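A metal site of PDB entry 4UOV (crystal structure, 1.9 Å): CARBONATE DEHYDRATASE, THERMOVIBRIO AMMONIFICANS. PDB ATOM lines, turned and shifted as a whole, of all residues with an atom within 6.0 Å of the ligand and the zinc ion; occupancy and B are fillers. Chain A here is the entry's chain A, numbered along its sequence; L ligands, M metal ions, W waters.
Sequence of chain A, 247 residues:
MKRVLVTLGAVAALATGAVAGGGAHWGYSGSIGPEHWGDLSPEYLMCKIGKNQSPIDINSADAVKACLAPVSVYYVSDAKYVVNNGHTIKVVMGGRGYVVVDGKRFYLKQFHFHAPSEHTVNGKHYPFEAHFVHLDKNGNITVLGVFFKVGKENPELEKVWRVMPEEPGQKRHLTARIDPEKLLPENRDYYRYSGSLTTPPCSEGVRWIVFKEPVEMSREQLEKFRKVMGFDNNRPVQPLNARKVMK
OE1 of Glu 118 touches N1 of the ligand, at 3.8 Å. CG2 of Val 133 touches O2 of the ligand, at 3.7 Å. Val 143 touches the ligand. Leu 197 touches the ligand. Trp 208 touches the ligand. Hydrophobic or aromatic side chains within 4 Å of the ligand: His 112, His 114, His 131, Val 133, Val 143, Leu 197 and Trp 208. 11 residues have an atom within 4 Å of the ligand: Gln 110, His 112, His 114, Glu 118, His 131, Val 133, Val 143, Leu 197, Thr 198, Thr 199 and Trp 208.
Merely in contact with the zinc ion: Glu 118. Four residues have an atom within 4 Å of the zinc ion: His 112, His 114, Glu 118 and His 131.
The side-chain carboxylate of Glu 118 lies close to a ring nitrogen (NE2) of His 114. OE1 of Gln 110 sits at hydrogen-bond distance from ND1 of His 112, 2.7 Å away. The side-chain hydroxyl (OG1) of Thr 198 is in hydrogen-bond range of the side-chain carboxylate (OE1) of Glu 118 (2.6 Å). The backbone carbonyl oxygen (O) of Gln 110 lies within hydrogen-bond range of the backbone NH (N) of Val 133, at 2.9 Å. The indole nitrogen of Trp 208 lies within hydrogen-bond range of the backbone carbonyl oxygen of Ser 196, 2.9 Å away.
A nitrogen (N2) of the ligand sits at hydrogen-bond distance from the side-chain hydroxyl of Thr 199 (2.7 Å). The backbone NH (N) of Thr 198 lies within hydrogen-bond range of an oxygen (O1) of the ligand (2.9 Å). N1 of the ligand lies close to OG1 of Thr 198. The side-chain amide nitrogen (NE2) of Gln 110 is in hydrogen-bond range of an oxygen (O3) of the ligand (2.9 Å).
N1 of the ligand binds the zinc ion (2.1 Å). NE2 of His 114 is bound to the zinc ion, 2.1 Å away. NE2 of His 112 binds the zinc ion (2.1 Å). ND1 of His 131 is bound to the zinc ion, at 2.1 Å. The zinc ion has four donor atoms within binding distance.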
ATOM      1  N   HIS A  87       6.400   2.961  19.635  1.00  0.00           N
ATOM      2  CA  HIS A  87       6.724   2.150  20.809  1.00  0.00           C
ATOM      3  C   HIS A  87       5.777   2.374  21.985  1.00  0.00           C
ATOM      4  O   HIS A  87       5.785   1.606  22.951  1.00  0.00           O
ATOM      5  CB  HIS A  87       8.232   2.229  21.201  1.00  0.00           C
ATOM      6  CG  HIS A  87       8.665   3.542  21.795  1.00  0.00           C
ATOM      7  ND1 HIS A  87       8.489   3.859  23.127  1.00  0.00           N
ATOM      8  CD2 HIS A  87       9.343   4.585  21.243  1.00  0.00           C
ATOM      9  CE1 HIS A  87       9.002   5.060  23.364  1.00  0.00           C
ATOM     10  NE2 HIS A  87       9.526   5.517  22.239  1.00  0.00           N
ATOM     11  N   LYS A  90       1.583   8.332  23.448  1.00  0.00           N
ATOM     12  CA  LYS A  90       2.128   9.381  24.302  1.00  0.00           C
ATOM     13  C   LYS A  90       1.358  10.684  24.168  1.00  0.00           C
ATOM     14  O   LYS A  90       1.130  11.185  23.055  1.00  0.00           O
ATOM     15  CB  LYS A  90       3.610   9.611  23.986  1.00  0.00           C
ATOM     16  CG  LYS A  90       4.193  10.886  24.588  1.00  0.00           C
ATOM     17  CD  LYS A  90       5.714  10.955  24.478  1.00  0.00           C
ATOM     18  CE  LYS A  90       6.170  11.128  23.045  1.00  0.00           C
ATOM     19  NZ  LYS A  90       7.656  11.238  22.963  1.00  0.00           N
ATOM     20  N   GLN A 110       5.320  14.893  29.421  1.00  0.00           N
ATOM     21  CA  GLN A 110       4.531  13.931  28.650  1.00  0.00           C
ATOM     22  C   GLN A 110       4.139  12.813  29.567  1.00  0.00           C
ATOM     23  O   GLN A 110       4.776  12.591  30.611  1.00  0.00           O
ATOM     24  CB  GLN A 110       5.361  13.356  27.463  1.00  0.00           C
ATOM     25  CG  GLN A 110       6.732  12.780  27.858  1.00  0.00           C
ATOM     26  CD  GLN A 110       6.802  11.268  27.810  1.00  0.00           C
ATOM     27  OE1 GLN A 110       5.822  10.565  28.081  1.00  0.00           O
ATOM     28  NE2 GLN A 110       7.983  10.741  27.466  1.00  0.00           N
ATOM     29  N   HIS A 112       2.797   8.493  29.051  1.00  0.00           N
ATOM     30  CA  HIS A 112       2.668   7.420  28.073  1.00  0.00           C
ATOM     31  C   HIS A 112       2.389   6.093  28.763  1.00  0.00           C
ATOM     32  O   HIS A 112       2.286   6.041  30.000  1.00  0.00           O
ATOM     33  CB  HIS A 112       3.932   7.324  27.221  1.00  0.00           C
ATOM     34  CG  HIS A 112       5.149   6.954  28.004  1.00  0.00           C
ATOM     35  ND1 HIS A 112       5.958   7.886  28.599  1.00  0.00           N
ATOM     36  CD2 HIS A 112       5.665   5.744  28.341  1.00  0.00           C
ATOM     37  CE1 HIS A 112       6.946   7.277  29.239  1.00  0.00           C
ATOM     38  NE2 HIS A 112       6.785   5.974  29.103  1.00  0.00           N
ATOM     39  N   PHE A 113       2.281   5.014  27.985  1.00  0.00           N
ATOM     40  CA  PHE A 113       1.710   3.779  28.501  1.00  0.00           C
ATOM     41  C   PHE A 113       2.435   2.498  28.077  1.00  0.00           C
ATOM     42  O   PHE A 113       2.975   2.413  26.960  1.00  0.00           O
ATOM     43  CB  PHE A 113       0.215   3.698  28.090  1.00  0.00           C
ATOM     44  CG  PHE A 113      -0.584   4.930  28.454  1.00  0.00           C
ATOM     45  CD1 PHE A 113      -1.150   5.065  29.711  1.00  0.00           C
ATOM     46  CD2 PHE A 113      -0.753   5.962  27.531  1.00  0.00           C
ATOM     47  CE1 PHE A 113      -1.886   6.202  30.053  1.00  0.00           C
ATOM     48  CE2 PHE A 113      -1.478   7.099  27.863  1.00  0.00           C
ATOM     49  CZ  PHE A 113      -2.041   7.226  29.123  1.00  0.00           C
ATOM     50  N   HIS A 114       2.398   1.491  28.966  1.00  0.00           N
ATOM     51  CA  HIS A 114       2.929   0.153  28.714  1.00  0.00           C
ATOM     52  C   HIS A 114       1.910  -0.932  29.054  1.00  0.00           C
ATOM     53  O   HIS A 114       1.148  -0.814  30.020  1.00  0.00           O
ATOM     54  CB  HIS A 114       4.225  -0.103  29.513  1.00  0.00           C
ATOM     55  CG  HIS A 114       5.289   0.946  29.311  1.00  0.00           C
ATOM     56  ND1 HIS A 114       6.331   0.794  28.421  1.00  0.00           N
ATOM     57  CD2 HIS A 114       5.473   2.150  29.906  1.00  0.00           C
ATOM     58  CE1 HIS A 114       7.097   1.869  28.462  1.00  0.00           C
ATOM     59  NE2 HIS A 114       6.616   2.694  29.372  1.00  0.00           N
ATOM     60  N   GLU A 118       5.490  -2.569  33.391  1.00  0.00           N
ATOM     61  CA  GLU A 118       6.947  -2.688  33.417  1.00  0.00           C
ATOM     62  C   GLU A 118       7.422  -3.126  34.807  1.00  0.00           C
ATOM     63  O   GLU A 118       8.146  -4.123  34.929  1.00  0.00           O
ATOM     64  CB  GLU A 118       7.604  -1.378  32.999  1.00  0.00           C
ATOM     65  CG  GLU A 118       7.240  -0.980  31.571  1.00  0.00           C
ATOM     66  CD  GLU A 118       8.387  -0.290  30.891  1.00  0.00           C
ATOM     67  OE1 GLU A 118       8.653   0.874  31.237  1.00  0.00           O
ATOM     68  OE2 GLU A 118       9.030  -0.900  29.997  1.00  0.00           O
ATOM     69  N   HIS A 131       3.177   6.098  32.752  1.00  0.00           N
ATOM     70  CA  HIS A 131       4.379   6.825  33.177  1.00  0.00           C
ATOM     71  C   HIS A 131       4.221   8.313  32.909  1.00  0.00           C
ATOM     72  O   HIS A 131       3.957   8.733  31.778  1.00  0.00           O
ATOM     73  CB  HIS A 131       5.644   6.304  32.471  1.00  0.00           C
ATOM     74  CG  HIS A 131       6.043   4.920  32.893  1.00  0.00           C
ATOM     75  ND1 HIS A 131       6.874   4.124  32.138  1.00  0.00           N
ATOM     76  CD2 HIS A 131       5.705   4.186  33.981  1.00  0.00           C
ATOM     77  CE1 HIS A 131       7.051   2.966  32.738  1.00  0.00           C
ATOM     78  NE2 HIS A 131       6.347   2.970  33.861  1.00  0.00           N
ATOM     79  N   VAL A 133       6.243  11.671  32.913  1.00  0.00           N
ATOM     80  CA  VAL A 133       7.678  11.973  32.803  1.00  0.00           C
ATOM     81  C   VAL A 133       7.935  13.445  33.059  1.00  0.00           C
ATOM     82  O   VAL A 133       7.361  14.312  32.387  1.00  0.00           O
ATOM     83  CB  VAL A 133       8.256  11.531  31.429  1.00  0.00           C
ATOM     84  CG1 VAL A 133       9.729  11.883  31.301  1.00  0.00           C
ATOM     85  CG2 VAL A 133       8.055  10.038  31.236  1.00  0.00           C
ATOM     86  N   VAL A 143      10.127  10.094  37.123  1.00  0.00           N
ATOM     87  CA  VAL A 143       8.972   9.415  36.539  1.00  0.00           C
ATOM     88  C   VAL A 143       8.002   8.943  37.638  1.00  0.00           C
ATOM     89  O   VAL A 143       8.410   8.301  38.621  1.00  0.00           O
ATOM     90  CB  VAL A 143       9.362   8.219  35.637  1.00  0.00           C
ATOM     91  CG1 VAL A 143       8.145   7.708  34.863  1.00  0.00           C
ATOM     92  CG2 VAL A 143      10.457   8.609  34.655  1.00  0.00           C
ATOM     93  N   SER A 196      16.547   4.107  36.204  1.00  0.00           N
ATOM     94  CA  SER A 196      16.909   4.523  34.859  1.00  0.00           C
ATOM     95  C   SER A 196      15.671   4.714  33.989  1.00  0.00           C
ATOM     96  O   SER A 196      14.569   4.364  34.393  1.00  0.00           O
ATOM     97  CB  SER A 196      17.817   3.467  34.213  1.00  0.00           C
ATOM     98  OG  SER A 196      17.068   2.368  33.694  1.00  0.00           O
ATOM     99  N   LEU A 197      15.851   5.274  32.794  1.00  0.00           N
ATOM    100  CA  LEU A 197      14.797   5.183  31.784  1.00  0.00           C
ATOM    101  C   LEU A 197      14.663   3.729  31.333  1.00  0.00           C
ATOM    102  O   LEU A 197      15.649   2.982  31.363  1.00  0.00           O
ATOM    103  CB  LEU A 197      15.124   6.097  30.613  1.00  0.00           C
ATOM    104  CG  LEU A 197      15.213   7.576  30.969  1.00  0.00           C
ATOM    105  CD1 LEU A 197      15.547   8.385  29.720  1.00  0.00           C
ATOM    106  CD2 LEU A 197      13.927   8.080  31.593  1.00  0.00           C
ATOM    107  N   THR A 198      13.466   3.315  30.902  1.00  0.00           N
ATOM    108  CA  THR A 198      13.246   1.918  30.520  1.00  0.00           C
ATOM    109  C   THR A 198      13.312   1.682  29.011  1.00  0.00           C
ATOM    110  O   THR A 198      13.071   0.562  28.555  1.00  0.00           O
ATOM    111  CB  THR A 198      11.896   1.364  31.049  1.00  0.00           C
ATOM    112  OG1 THR A 198      10.809   2.001  30.349  1.00  0.00           O
ATOM    113  CG2 THR A 198      11.735   1.597  32.577  1.00  0.00           C
ATOM    114  N   THR A 199      13.608   2.712  28.234  1.00  0.00           N
ATOM    115  CA  THR A 199      13.935   2.535  26.809  1.00  0.00           C
ATOM    116  C   THR A 199      15.341   3.062  26.521  1.00  0.00           C
ATOM    117  O   THR A 199      15.814   3.967  27.241  1.00  0.00           O
ATOM    118  CB  THR A 199      12.920   3.254  25.883  1.00  0.00           C
ATOM    119  OG1 THR A 199      12.997   4.670  26.097  1.00  0.00           O
ATOM    120  CG2 THR A 199      11.505   2.787  26.167  1.00  0.00           C
ATOM    121  N   PRO A 200      16.025   2.516  25.494  1.00  0.00           N
ATOM    122  CA  PRO A 200      17.368   3.015  25.172  1.00  0.00           C
ATOM    123  C   PRO A 200      17.399   4.539  25.066  1.00  0.00           C
ATOM    124  O   PRO A 200      16.466   5.124  24.522  1.00  0.00           O
ATOM    125  CB  PRO A 200      17.666   2.360  23.808  1.00  0.00           C
ATOM    126  CG  PRO A 200      16.895   1.084  23.872  1.00  0.00           C
ATOM    127  CD  PRO A 200      15.616   1.455  24.558  1.00  0.00           C
ATOM    128  N   TRP A 208      12.332   7.393  40.652  1.00  0.00           N
ATOM    129  CA  TRP A 208      11.088   6.665  40.397  1.00  0.00           C
ATOM    130  C   TRP A 208      10.148   6.766  41.591  1.00  0.00           C
ATOM    131  O   TRP A 208      10.543   6.462  42.724  1.00  0.00           O
ATOM    132  CB  TRP A 208      11.335   5.184  40.056  1.00  0.00           C
ATOM    133  CG  TRP A 208      11.658   4.988  38.604  1.00  0.00           C
ATOM    134  CD1 TRP A 208      12.906   4.985  38.039  1.00  0.00           C
ATOM    135  CD2 TRP A 208      10.728   4.853  37.527  1.00  0.00           C
ATOM    136  NE1 TRP A 208      12.805   4.813  36.679  1.00  0.00           N
ATOM    137  CE2 TRP A 208      11.477   4.725  36.334  1.00  0.00           C
ATOM    138  CE3 TRP A 208       9.326   4.806  37.462  1.00  0.00           C
ATOM    139  CZ2 TRP A 208      10.875   4.555  35.071  1.00  0.00           C
ATOM    140  CZ3 TRP A 208       8.718   4.623  36.201  1.00  0.00           C
ATOM    141  CH2 TRP A 208       9.495   4.500  35.032  1.00  0.00           C
HETATM  142  C1  LIG L   1      11.041   6.516  29.453  1.00  0.00           C
HETATM  143  C2  LIG L   1      11.876   7.914  27.769  1.00  0.00           C
HETATM  144  C3  LIG L   1      11.678  10.056  26.628  1.00  0.00           C
HETATM  145  C4  LIG L   1      12.023  10.741  25.345  1.00  0.00           C
HETATM  146  N1  LIG L   1       9.610   4.382  30.177  1.00  0.00           N
HETATM  147  N2  LIG L   1      12.375   6.704  27.711  1.00  0.00           N
HETATM  148  N3  LIG L   1      11.888   5.899  28.702  1.00  0.00           N
HETATM  149  N4  LIG L   1      12.259   8.839  26.820  1.00  0.00           N
HETATM  150  O1  LIG L   1      11.409   5.249  31.591  1.00  0.00           O
HETATM  151  O2  LIG L   1       9.293   6.567  31.355  1.00  0.00           O
HETATM  152  O3  LIG L   1      10.924  10.532  27.474  1.00  0.00           O
HETATM  153  S1  LIG L   1      10.289   5.674  30.819  1.00  0.00           S
HETATM  154  S2  LIG L   1      10.743   8.173  29.046  1.00  0.00           S
HETATM  155 ZN    ZN M   1       7.558   4.352  30.155  1.00  0.00          ZN
HETATM  156  O   HOH W   1      15.271   6.763  26.736  1.00  0.00           O
